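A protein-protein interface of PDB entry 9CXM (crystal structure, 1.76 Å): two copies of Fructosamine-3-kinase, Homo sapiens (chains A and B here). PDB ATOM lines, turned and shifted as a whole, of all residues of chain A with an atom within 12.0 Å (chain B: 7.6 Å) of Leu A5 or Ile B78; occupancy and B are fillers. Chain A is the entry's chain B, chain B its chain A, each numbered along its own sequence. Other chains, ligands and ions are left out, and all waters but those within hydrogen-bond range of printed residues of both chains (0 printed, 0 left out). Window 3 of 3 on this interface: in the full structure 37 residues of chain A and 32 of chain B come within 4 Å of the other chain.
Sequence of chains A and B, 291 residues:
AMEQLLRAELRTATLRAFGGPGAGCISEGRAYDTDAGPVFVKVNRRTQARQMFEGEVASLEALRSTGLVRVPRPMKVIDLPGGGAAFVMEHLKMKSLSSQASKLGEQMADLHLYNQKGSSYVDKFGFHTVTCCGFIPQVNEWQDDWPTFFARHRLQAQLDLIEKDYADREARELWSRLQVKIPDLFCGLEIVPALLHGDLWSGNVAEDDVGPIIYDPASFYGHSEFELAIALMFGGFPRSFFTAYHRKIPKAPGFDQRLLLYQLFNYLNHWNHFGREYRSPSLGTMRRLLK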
ATOM      1  N   ALA A   1     -27.803  -5.216 -18.430  1.00  0.00           N
ATOM      2  CA  ALA A   1     -29.208  -5.628 -18.227  1.00  0.00           C
ATOM      3  C   ALA A   1     -29.340  -7.140 -18.415  1.00  0.00           C
ATOM      4  O   ALA A   1     -28.374  -7.765 -18.887  1.00  0.00           O
ATOM      5  CB  ALA A   1     -30.097  -4.880 -19.190  1.00  0.00           C
ATOM      6  N   MET A   2     -30.508  -7.695 -18.080  1.00  0.00           N
ATOM      7  CA  MET A   2     -30.747  -9.144 -18.291  1.00  0.00           C
ATOM      8  C   MET A   2     -30.565  -9.443 -19.774  1.00  0.00           C
ATOM      9  O   MET A   2     -29.958 -10.466 -20.102  1.00  0.00           O
ATOM     10  CB  MET A   2     -32.169  -9.527 -17.878  1.00  0.00           C
ATOM     11  CG  MET A   2     -32.303  -9.884 -16.414  1.00  0.00           C
ATOM     12  SD  MET A   2     -31.637 -11.529 -16.073  1.00  0.00           S
ATOM     13  CE  MET A   2     -32.318 -12.445 -17.452  1.00  0.00           C
ATOM     14  N   GLU A   3     -31.065  -8.552 -20.628  1.00  0.00           N
ATOM     15  CA  GLU A   3     -30.935  -8.750 -22.089  1.00  0.00           C
ATOM     16  C   GLU A   3     -29.456  -8.901 -22.439  1.00  0.00           C
ATOM     17  O   GLU A   3     -29.118  -9.841 -23.171  1.00  0.00           O
ATOM     18  CB  GLU A   3     -31.558  -7.566 -22.828  1.00  0.00           C
ATOM     19  CG  GLU A   3     -32.671  -7.958 -23.783  1.00  0.00           C
ATOM     20  CD  GLU A   3     -34.044  -7.406 -23.441  1.00  0.00           C
ATOM     21  OE1 GLU A   3     -34.926  -7.430 -24.322  1.00  0.00           O
ATOM     22  OE2 GLU A   3     -34.234  -6.960 -22.292  1.00  0.00           O
ATOM     23  N   GLN A   4     -28.611  -8.005 -21.929  1.00  0.00           N
ATOM     24  CA  GLN A   4     -27.163  -8.047 -22.263  1.00  0.00           C
ATOM     25  C   GLN A   4     -26.563  -9.362 -21.762  1.00  0.00           C
ATOM     26  O   GLN A   4     -25.819 -10.000 -22.519  1.00  0.00           O
ATOM     27  CB  GLN A   4     -26.464  -6.836 -21.645  1.00  0.00           C
ATOM     28  CG  GLN A   4     -27.129  -5.517 -22.008  1.00  0.00           C
ATOM     29  CD  GLN A   4     -27.171  -5.305 -23.502  1.00  0.00           C
ATOM     30  OE1 GLN A   4     -26.361  -5.848 -24.249  1.00  0.00           O
ATOM     31  NE2 GLN A   4     -28.122  -4.503 -23.951  1.00  0.00           N
ATOM     32  N   LEU A   5     -26.899  -9.747 -20.534  1.00  0.00           N
ATOM     33  CA  LEU A   5     -26.370 -11.006 -19.950  1.00  0.00           C
ATOM     34  C   LEU A   5     -26.854 -12.198 -20.787  1.00  0.00           C
ATOM     35  O   LEU A   5     -26.046 -13.088 -21.062  1.00  0.00           O
ATOM     36  CB  LEU A   5     -26.839 -11.107 -18.496  1.00  0.00           C
ATOM     37  CG  LEU A   5     -26.205 -12.225 -17.672  1.00  0.00           C
ATOM     38  CD1 LEU A   5     -24.703 -12.020 -17.553  1.00  0.00           C
ATOM     39  CD2 LEU A   5     -26.839 -12.300 -16.293  1.00  0.00           C
ATOM     40  N   LEU A   6     -28.126 -12.184 -21.188  1.00  0.00           N
ATOM     41  CA  LEU A   6     -28.684 -13.312 -21.978  1.00  0.00           C
ATOM     42  C   LEU A   6     -28.022 -13.343 -23.359  1.00  0.00           C
ATOM     43  O   LEU A   6     -27.583 -14.421 -23.774  1.00  0.00           O
ATOM     44  CB  LEU A   6     -30.207 -13.166 -22.068  1.00  0.00           C
ATOM     45  CG  LEU A   6     -30.964 -13.395 -20.763  1.00  0.00           C
ATOM     46  CD1 LEU A   6     -32.458 -13.195 -20.964  1.00  0.00           C
ATOM     47  CD2 LEU A   6     -30.685 -14.785 -20.214  1.00  0.00           C
ATOM     48  N   ARG A   7     -27.913 -12.187 -24.013  1.00  0.00           N
ATOM     49  CA  ARG A   7     -27.253 -12.127 -25.340  1.00  0.00           C
ATOM     50  C   ARG A   7     -25.841 -12.696 -25.211  1.00  0.00           C
ATOM     51  O   ARG A   7     -25.405 -13.406 -26.125  1.00  0.00           O
ATOM     52  CB  ARG A   7     -27.207 -10.687 -25.860  1.00  0.00           C
ATOM     53  CG  ARG A   7     -28.545 -10.125 -26.316  1.00  0.00           C
ATOM     54  CD  ARG A   7     -28.341  -8.826 -27.075  1.00  0.00           C
ATOM     55  NE  ARG A   7     -29.575  -8.242 -27.578  1.00  0.00           N
ATOM     56  CZ  ARG A   7     -30.299  -7.339 -26.927  1.00  0.00           C
ATOM     57  NH1 ARG A   7     -29.909  -6.910 -25.739  1.00  0.00           N
ATOM     58  NH2 ARG A   7     -31.407  -6.865 -27.465  1.00  0.00           N
ATOM     59  N   ALA A   8     -25.168 -12.393 -24.101  1.00  0.00           N
ATOM     60  CA  ALA A   8     -23.786 -12.872 -23.887  1.00  0.00           C
ATOM     61  C   ALA A   8     -23.785 -14.344 -23.484  1.00  0.00           C
ATOM     62  O   ALA A   8     -22.985 -15.103 -24.041  1.00  0.00           O
ATOM     63  CB  ALA A   8     -23.133 -12.031 -22.824  1.00  0.00           C
ATOM     64  N   GLU A   9     -24.638 -14.723 -22.537  1.00  0.00           N
ATOM     65  CA  GLU A   9     -24.595 -16.090 -22.050  1.00  0.00           C
ATOM     66  C   GLU A   9     -25.046 -17.076 -23.119  1.00  0.00           C
ATOM     67  O   GLU A   9     -24.547 -18.206 -23.174  1.00  0.00           O
ATOM     68  CB  GLU A   9     -25.474 -16.232 -20.810  1.00  0.00           C
ATOM     69  CG  GLU A   9     -24.971 -15.461 -19.596  1.00  0.00           C
ATOM     70  CD  GLU A   9     -23.858 -16.192 -18.909  1.00  0.00           C
ATOM     71  OE1 GLU A   9     -23.675 -17.389 -19.218  1.00  0.00           O
ATOM     72  OE2 GLU A   9     -23.171 -15.574 -18.070  1.00  0.00           O
ATOM     73  N   LEU A  10     -26.026 -16.687 -23.927  1.00  0.00           N
ATOM     74  CA  LEU A  10     -26.554 -17.546 -24.984  1.00  0.00           C
ATOM     75  C   LEU A  10     -25.915 -17.306 -26.347  1.00  0.00           C
ATOM     76  O   LEU A  10     -26.017 -18.184 -27.214  1.00  0.00           O
ATOM     77  CB  LEU A  10     -28.079 -17.359 -25.112  1.00  0.00           C
ATOM     78  CG  LEU A  10     -28.910 -17.632 -23.838  1.00  0.00           C
ATOM     79  CD1 LEU A  10     -30.397 -17.327 -24.035  1.00  0.00           C
ATOM     80  CD2 LEU A  10     -28.698 -19.039 -23.312  1.00  0.00           C
ATOM     81  N   ARG A  11     -25.206 -16.181 -26.530  1.00  0.00           N
ATOM     82  CA  ARG A  11     -24.549 -15.825 -27.789  1.00  0.00           C
ATOM     83  C   ARG A  11     -25.545 -15.567 -28.922  1.00  0.00           C
ATOM     84  O   ARG A  11     -25.493 -16.217 -29.959  1.00  0.00           O
ATOM     85  CB  ARG A  11     -23.540 -16.916 -28.153  1.00  0.00           C
ATOM     86  CG  ARG A  11     -22.671 -17.346 -26.954  1.00  0.00           C
ATOM     87  CD  ARG A  11     -21.564 -18.313 -27.349  1.00  0.00           C
ATOM     88  NE  ARG A  11     -21.079 -19.137 -26.241  1.00  0.00           N
ATOM     89  CZ  ARG A  11     -20.015 -18.872 -25.487  1.00  0.00           C
ATOM     90  NH1 ARG A  11     -19.262 -17.804 -25.696  1.00  0.00           N
ATOM     91  NH2 ARG A  11     -19.687 -19.713 -24.507  1.00  0.00           N
ATOM     92  N   THR A  12     -26.427 -14.590 -28.736  1.00  0.00           N
ATOM     93  CA  THR A  12     -27.475 -14.224 -29.685  1.00  0.00           C
ATOM     94  C   THR A  12     -27.437 -12.728 -29.966  1.00  0.00           C
ATOM     95  O   THR A  12     -27.219 -11.922 -29.050  1.00  0.00           O
ATOM     96  CB  THR A  12     -28.892 -14.604 -29.161  1.00  0.00           C
ATOM     97  OG1 THR A  12     -29.910 -14.043 -30.015  1.00  0.00           O
ATOM     98  CG2 THR A  12     -29.117 -14.094 -27.730  1.00  0.00           C
ATOM     99  N   ALA A  13     -27.676 -12.352 -31.233  1.00  0.00           N
ATOM    100  CA  ALA A  13     -27.723 -10.929 -31.561  1.00  0.00           C
ATOM    101  C   ALA A  13     -28.998 -10.265 -31.040  1.00  0.00           C
ATOM    102  O   ALA A  13     -28.940  -9.338 -30.220  1.00  0.00           O
ATOM    103  CB  ALA A  13     -27.601 -10.740 -33.072  1.00  0.00           C
ATOM    104  N   THR A  14     -30.148 -10.799 -31.458  1.00  0.00           N
ATOM    105  CA  THR A  14     -31.445 -10.195 -31.052  1.00  0.00           C
ATOM    106  C   THR A  14     -32.033 -10.918 -29.840  1.00  0.00           C
ATOM    107  O   THR A  14     -31.646 -12.074 -29.593  1.00  0.00           O
ATOM    108  CB  THR A  14     -32.446 -10.202 -32.212  1.00  0.00           C
ATOM    109  OG1 THR A  14     -32.652 -11.564 -32.591  1.00  0.00           O
ATOM    110  CG2 THR A  14     -31.973  -9.396 -33.401  1.00  0.00           C
ATOM    111  N   LEU A  15     -32.924 -10.239 -29.116  1.00  0.00           N
ATOM    112  CA  LEU A  15     -33.587 -10.833 -27.932  1.00  0.00           C
ATOM    113  C   LEU A  15     -34.827  -9.983 -27.642  1.00  0.00           C
ATOM    114  O   LEU A  15     -34.669  -8.913 -27.027  1.00  0.00           O
ATOM    115  CB  LEU A  15     -32.610 -10.814 -26.753  1.00  0.00           C
ATOM    116  CG  LEU A  15     -32.921 -11.792 -25.623  1.00  0.00           C
ATOM    117  CD1 LEU A  15     -32.379 -13.174 -25.952  1.00  0.00           C
ATOM    118  CD2 LEU A  15     -32.338 -11.298 -24.311  1.00  0.00           C
ATOM    119  N   ARG A  16     -36.008 -10.427 -28.084  1.00  0.00           N
ATOM    120  CA  ARG A  16     -37.226  -9.590 -27.923  1.00  0.00           C
ATOM    121  C   ARG A  16     -38.228 -10.294 -27.010  1.00  0.00           C
ATOM    122  O   ARG A  16     -38.675 -11.393 -27.367  1.00  0.00           O
ATOM    123  CB  ARG A  16     -37.853  -9.287 -29.287  1.00  0.00           C
ATOM    124  N   VAL B  41     -37.102 -18.000 -19.908  1.00  0.00           N
ATOM    125  CA  VAL B  41     -36.137 -17.684 -18.867  1.00  0.00           C
ATOM    126  C   VAL B  41     -36.902 -17.473 -17.592  1.00  0.00           C
ATOM    127  O   VAL B  41     -37.801 -16.620 -17.537  1.00  0.00           O
ATOM    128  CB  VAL B  41     -35.304 -16.421 -19.214  1.00  0.00           C
ATOM    129  CG1 VAL B  41     -34.280 -16.215 -18.127  1.00  0.00           C
ATOM    130  CG2 VAL B  41     -34.649 -16.585 -20.528  1.00  0.00           C
ATOM    131  N   LYS B  42     -36.541 -18.223 -16.536  1.00  0.00           N
ATOM    132  CA  LYS B  42     -37.078 -18.023 -15.202  1.00  0.00           C
ATOM    133  C   LYS B  42     -36.061 -17.267 -14.371  1.00  0.00           C
ATOM    134  O   LYS B  42     -34.871 -17.562 -14.404  1.00  0.00           O
ATOM    135  CB  LYS B  42     -37.422 -19.342 -14.452  1.00  0.00           C
ATOM    136  CG  LYS B  42     -38.644 -20.092 -14.978  1.00  0.00           C
ATOM    137  CD  LYS B  42     -38.569 -21.611 -14.522  1.00  0.00           C
ATOM    138  CE  LYS B  42     -39.714 -21.961 -13.655  1.00  0.00           C
ATOM    139  NZ  LYS B  42     -39.782 -23.415 -13.331  1.00  0.00           N
ATOM    140  N   ASN B  44     -35.071 -15.681 -10.508  1.00  0.00           N
ATOM    141  CA  ASN B  44     -35.347 -15.713  -9.089  1.00  0.00           C
ATOM    142  C   ASN B  44     -34.211 -14.994  -8.403  1.00  0.00           C
ATOM    143  O   ASN B  44     -33.057 -15.418  -8.516  1.00  0.00           O
ATOM    144  CB  ASN B  44     -35.462 -17.134  -8.545  1.00  0.00           C
ATOM    145  CG  ASN B  44     -35.883 -17.158  -7.089  1.00  0.00           C
ATOM    146  OD1 ASN B  44     -35.162 -16.719  -6.191  1.00  0.00           O
ATOM    147  ND2 ASN B  44     -37.092 -17.635  -6.856  1.00  0.00           N
ATOM    148  N   ALA B  49     -31.402 -19.275  -5.209  1.00  0.00           N
ATOM    149  CA  ALA B  49     -31.978 -19.526  -6.532  1.00  0.00           C
ATOM    150  C   ALA B  49     -31.182 -20.578  -7.309  1.00  0.00           C
ATOM    151  O   ALA B  49     -31.778 -21.480  -7.933  1.00  0.00           O
ATOM    152  CB  ALA B  49     -32.090 -18.213  -7.310  1.00  0.00           C
ATOM    153  N   ARG B  50     -29.843 -20.504  -7.275  1.00  0.00           N
ATOM    154  CA  ARG B  50     -29.035 -21.470  -8.038  1.00  0.00           C
ATOM    155  C   ARG B  50     -29.309 -22.890  -7.565  1.00  0.00           C
ATOM    156  O   ARG B  50     -29.574 -23.786  -8.377  1.00  0.00           O
ATOM    157  CB  ARG B  50     -27.529 -21.168  -7.941  1.00  0.00           C
ATOM    158  CG  ARG B  50     -26.684 -22.294  -8.497  1.00  0.00           C
ATOM    159  CD  ARG B  50     -25.211 -21.995  -8.882  1.00  0.00           C
ATOM    160  NE  ARG B  50     -24.994 -21.194 -10.079  1.00  0.00           N
ATOM    161  CZ  ARG B  50     -24.900 -21.679 -11.316  1.00  0.00           C
ATOM    162  NH1 ARG B  50     -25.084 -22.962 -11.572  1.00  0.00           N
ATOM    163  NH2 ARG B  50     -24.641 -20.853 -12.324  1.00  0.00           N
ATOM    164  N   PHE B  53     -32.649 -23.973  -8.830  1.00  0.00           N
ATOM    165  CA  PHE B  53     -32.672 -24.260 -10.250  1.00  0.00           C
ATOM    166  C   PHE B  53     -31.866 -25.511 -10.571  1.00  0.00           C
ATOM    167  O   PHE B  53     -32.242 -26.267 -11.489  1.00  0.00           O
ATOM    168  CB  PHE B  53     -32.149 -23.037 -11.005  1.00  0.00           C
ATOM    169  CG  PHE B  53     -33.158 -21.923 -11.144  1.00  0.00           C
ATOM    170  CD1 PHE B  53     -34.500 -22.176 -11.399  1.00  0.00           C
ATOM    171  CD2 PHE B  53     -32.749 -20.592 -11.017  1.00  0.00           C
ATOM    172  CE1 PHE B  53     -35.422 -21.120 -11.558  1.00  0.00           C
ATOM    173  CE2 PHE B  53     -33.668 -19.530 -11.179  1.00  0.00           C
ATOM    174  CZ  PHE B  53     -34.992 -19.777 -11.470  1.00  0.00           C
ATOM    175  N   MET B  75     -31.294 -25.421 -20.480  1.00  0.00           N
ATOM    176  CA  MET B  75     -30.146 -24.902 -21.227  1.00  0.00           C
ATOM    177  C   MET B  75     -29.061 -24.322 -20.335  1.00  0.00           C
ATOM    178  O   MET B  75     -27.903 -24.723 -20.451  1.00  0.00           O
ATOM    179  CB  MET B  75     -30.592 -23.863 -22.236  1.00  0.00           C
ATOM    180  CG  MET B  75     -31.619 -24.474 -23.195  1.00  0.00           C
ATOM    181  SD  MET B  75     -32.352 -23.265 -24.264  1.00  0.00           S
ATOM    182  CE  MET B  75     -30.908 -22.258 -24.727  1.00  0.00           C
ATOM    183  N   LYS B  76     -29.400 -23.415 -19.425  1.00  0.00           N
ATOM    184  CA  LYS B  76     -28.297 -22.805 -18.690  1.00  0.00           C
ATOM    185  C   LYS B  76     -28.803 -22.246 -17.383  1.00  0.00           C
ATOM    186  O   LYS B  76     -29.916 -21.741 -17.331  1.00  0.00           O
ATOM    187  CB  LYS B  76     -27.662 -21.670 -19.518  1.00  0.00           C
ATOM    188  CG  LYS B  76     -26.216 -21.443 -19.155  1.00  0.00           C
ATOM    189  CD  LYS B  76     -25.560 -20.503 -20.140  1.00  0.00           C
ATOM    190  CE  LYS B  76     -24.064 -20.838 -20.271  1.00  0.00           C
ATOM    191  NZ  LYS B  76     -23.285 -19.686 -20.841  1.00  0.00           N
ATOM    192  N   VAL B  77     -27.968 -22.310 -16.337  1.00  0.00           N
ATOM    193  CA  VAL B  77     -28.237 -21.611 -15.074  1.00  0.00           C
ATOM    194  C   VAL B  77     -27.160 -20.531 -14.892  1.00  0.00           C
ATOM    195  O   VAL B  77     -25.964 -20.845 -14.847  1.00  0.00           O
ATOM    196  CB  VAL B  77     -28.270 -22.573 -13.878  1.00  0.00           C
ATOM    197  CG1 VAL B  77     -28.418 -21.777 -12.611  1.00  0.00           C
ATOM    198  CG2 VAL B  77     -29.457 -23.609 -14.047  1.00  0.00           C
ATOM    199  N   ILE B  78     -27.596 -19.283 -14.731  1.00  0.00           N
ATOM    200  CA  ILE B  78     -26.731 -18.110 -14.797  1.00  0.00           C
ATOM    201  C   ILE B  78     -26.810 -17.374 -13.457  1.00  0.00           C
ATOM    202  O   ILE B  78     -27.908 -17.032 -12.989  1.00  0.00           O
ATOM    203  CB  ILE B  78     -27.179 -17.168 -15.924  1.00  0.00           C
ATOM    204  CG1 ILE B  78     -27.048 -17.854 -17.265  1.00  0.00           C
ATOM    205  CG2 ILE B  78     -26.349 -15.896 -15.921  1.00  0.00           C
ATOM    206  CD1 ILE B  78     -27.998 -17.273 -18.297  1.00  0.00           C
ATOM    207  N   ASP B  79     -25.660 -17.120 -12.850  1.00  0.00           N
ATOM    208  CA  ASP B  79     -25.651 -16.320 -11.635  1.00  0.00           C
ATOM    209  C   ASP B  79     -25.877 -14.869 -12.006  1.00  0.00           C
ATOM    210  O   ASP B  79     -25.282 -14.359 -12.959  1.00  0.00           O
ATOM    211  CB  ASP B  79     -24.331 -16.496 -10.900  1.00  0.00           C
ATOM    212  CG  ASP B  79     -24.066 -17.922 -10.560  1.00  0.00           C
ATOM    213  OD1 ASP B  79     -24.804 -18.480  -9.704  1.00  0.00           O
ATOM    214  OD2 ASP B  79     -23.157 -18.506 -11.212  1.00  0.00           O
ATOM    215  N   LEU B  80     -26.763 -14.187 -11.235  1.00  0.00           N
ATOM    216  CA  LEU B  80     -27.188 -12.831 -11.540  1.00  0.00           C
ATOM    217  C   LEU B  80     -26.397 -11.834 -10.706  1.00  0.00           C
ATOM    218  O   LEU B  80     -26.271 -12.017  -9.488  1.00  0.00           O
ATOM    219  CB  LEU B  80     -28.681 -12.677 -11.264  1.00  0.00           C
ATOM    220  CG  LEU B  80     -29.629 -13.379 -12.248  1.00  0.00           C
ATOM    221  CD1 LEU B  80     -31.085 -13.075 -11.924  1.00  0.00           C
ATOM    222  CD2 LEU B  80     -29.349 -12.998 -13.695  1.00  0.00           C
ATOM    223  N   PRO B  81     -25.829 -10.794 -11.316  1.00  0.00           N
ATOM    224  CA  PRO B  81     -25.281  -9.686 -10.521  1.00  0.00           C
ATOM    225  C   PRO B  81     -26.309  -9.185  -9.517  1.00  0.00           C
ATOM    226  O   PRO B  81     -27.461  -8.894  -9.861  1.00  0.00           O
ATOM    227  CB  PRO B  81     -24.947  -8.610 -11.563  1.00  0.00           C
ATOM    228  CG  PRO B  81     -25.145  -9.214 -12.910  1.00  0.00           C
ATOM    229  CD  PRO B  81     -25.785 -10.563 -12.773  1.00  0.00           C
ATOM    230  N   GLY B  83     -27.407 -10.987  -7.027  1.00  0.00           N
ATOM    231  CA  GLY B  83     -27.965 -12.102  -6.289  1.00  0.00           C
ATOM    232  C   GLY B  83     -29.027 -12.853  -7.082  1.00  0.00           C
ATOM    233  O   GLY B  83     -29.786 -12.275  -7.874  1.00  0.00           O
ATOM    234  N   GLY B  84     -29.114 -14.162  -6.826  1.00  0.00           N
ATOM    235  CA  GLY B  84     -30.100 -14.966  -7.510  1.00  0.00           C
ATOM    236  C   GLY B  84     -29.552 -15.511  -8.813  1.00  0.00           C
ATOM    237  O   GLY B  84     -28.347 -15.522  -9.078  1.00  0.00           O
ATOM    238  N   ALA B  85     -30.471 -15.990  -9.635  1.00  0.00           N
ATOM    239  CA  ALA B  85     -30.053 -16.730 -10.821  1.00  0.00           C
ATOM    240  C   ALA B  85     -31.181 -16.691 -11.835  1.00  0.00           C
ATOM    241  O   ALA B  85     -32.340 -16.396 -11.511  1.00  0.00           O
ATOM    242  CB  ALA B  85     -29.640 -18.167 -10.435  1.00  0.00           C
ATOM    243  N   ALA B  86     -30.818 -16.928 -13.082  1.00  0.00           N
ATOM    244  CA  ALA B  86     -31.769 -17.114 -14.160  1.00  0.00           C
ATOM    245  C   ALA B  86     -31.572 -18.542 -14.670  1.00  0.00           C
ATOM    246  O   ALA B  86     -30.451 -19.057 -14.680  1.00  0.00           O
ATOM    247  CB  ALA B  86     -31.591 -16.123 -15.267  1.00  0.00           C
ATOM    248  N   PHE B  87     -32.665 -19.177 -15.061  1.00  0.00           N
ATOM    249  CA  PHE B  87     -32.649 -20.537 -15.607  1.00  0.00           C
ATOM    250  C   PHE B  87     -33.267 -20.440 -16.985  1.00  0.00           C
ATOM    251  O   PHE B  87     -34.420 -20.041 -17.125  1.00  0.00           O
ATOM    252  CB  PHE B  87     -33.418 -21.485 -14.661  1.00  0.00           C
ATOM    253  CG  PHE B  87     -33.647 -22.863 -15.241  1.00  0.00           C
ATOM    254  CD1 PHE B  87     -32.727 -23.418 -16.096  1.00  0.00           C
ATOM    255  CD2 PHE B  87     -34.795 -23.560 -14.919  1.00  0.00           C
ATOM    256  CE1 PHE B  87     -32.954 -24.697 -16.661  1.00  0.00           C
ATOM    257  CE2 PHE B  87     -35.051 -24.844 -15.478  1.00  0.00           C
ATOM    258  CZ  PHE B  87     -34.122 -25.398 -16.346  1.00  0.00           C
ATOM    259  N   VAL B  88     -32.469 -20.710 -18.007  1.00  0.00           N
ATOM    260  CA  VAL B  88     -32.897 -20.621 -19.394  1.00  0.00           C
ATOM    261  C   VAL B  88     -33.211 -22.037 -19.865  1.00  0.00           C
ATOM    262  O   VAL B  88     -32.384 -22.947 -19.673  1.00  0.00           O
ATOM    263  CB  VAL B  88     -31.806 -20.007 -20.278  1.00  0.00           C
ATOM    264  CG1 VAL B  88     -32.338 -19.873 -21.677  1.00  0.00           C
ATOM    265  CG2 VAL B  88     -31.367 -18.642 -19.712  1.00  0.00           C
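The side-chain carboxylate (OE1) of Glu A9 is in salt-bridge range of the side-chain amino group (NZ) of Lys B76 (2.8 Å).
O of Lys B76 sits at hydrogen-bond distance from N of Val B88.
The backbone carbonyl oxygen of Val B88 lies within hydrogen-bond range of the backbone NH of Met B75 (2.8 Å).
N of Ile B78 lies within hydrogen-bond range of O of Ala B86, 2.9 Å away.
Among the printed residues, merely in contact across the chains: Met A2 with Leu B80 (3.6 Å), Leu A5 with Ile B78 (3.6 Å), Leu A5 with Leu B80 (3.7 Å), Glu A9 with Ile B78 (3.7 Å), Leu A6 with Val B88 (3.9 Å) and Leu A10 with Val B88 (3.98 Å).
Of the printed residues of chain B, Leu A5 touches Ile B78 (3.6 Å) and Leu B80 (3.7 Å).
Of chain A, only Leu A5 (3.6 Å) and Glu A9 (3.7 Å) come within 4 Å of Ile B78.
Lys B76 touches just one residue of chain A: Glu A9.
No residue of chain A comes within 4 Å of Val B77.
No residue of chain A comes within 4 Å of Asp B79.
Leu B80 touches just these residues of chain A: Met A2 and Leu A5.
No residue of chain A comes within 4 Å of Gly B84.
No residue of chain A comes within 4 Å of Ala B85.
Of chain A, only Leu A6 (3.9 Å) and Leu A10 (3.98 Å) come within 4 Å of Val B88.
Printed residues of chain B within 4 Å of Glu A9: Lys B76 (2.8 Å) and Ile B78 (3.7 Å).
Printed residues of chain B within 4 Å of Leu A10: Val B88.
Of the printed residues of chain B, Leu A6 touches Val B88 (3.9 Å).
Of the printed residues of chain B, Met A2 touches Leu B80.
Ala B49 touches none of the printed residues of chain A.
Glu A3 touches none of the printed residues of chain B.
The nearest printed residue of chain B that does not touch Leu A6 is Val B41 (4.1 Å).
Of the 19 printed residues of chain B, 4 touch a printed residue of chain A.
Along chain B the printed residues that touch a printed residue of chain A span positions 76 to 88.
Among the printed residues, 7 pairs touch across the chains.
Among the printed residues, Asp or Glu carboxylates within 4 Å of a Lys or Arg side-chain nitrogen of the other chain: Glu A9 with Lys B76.
No position is printed for both chains.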
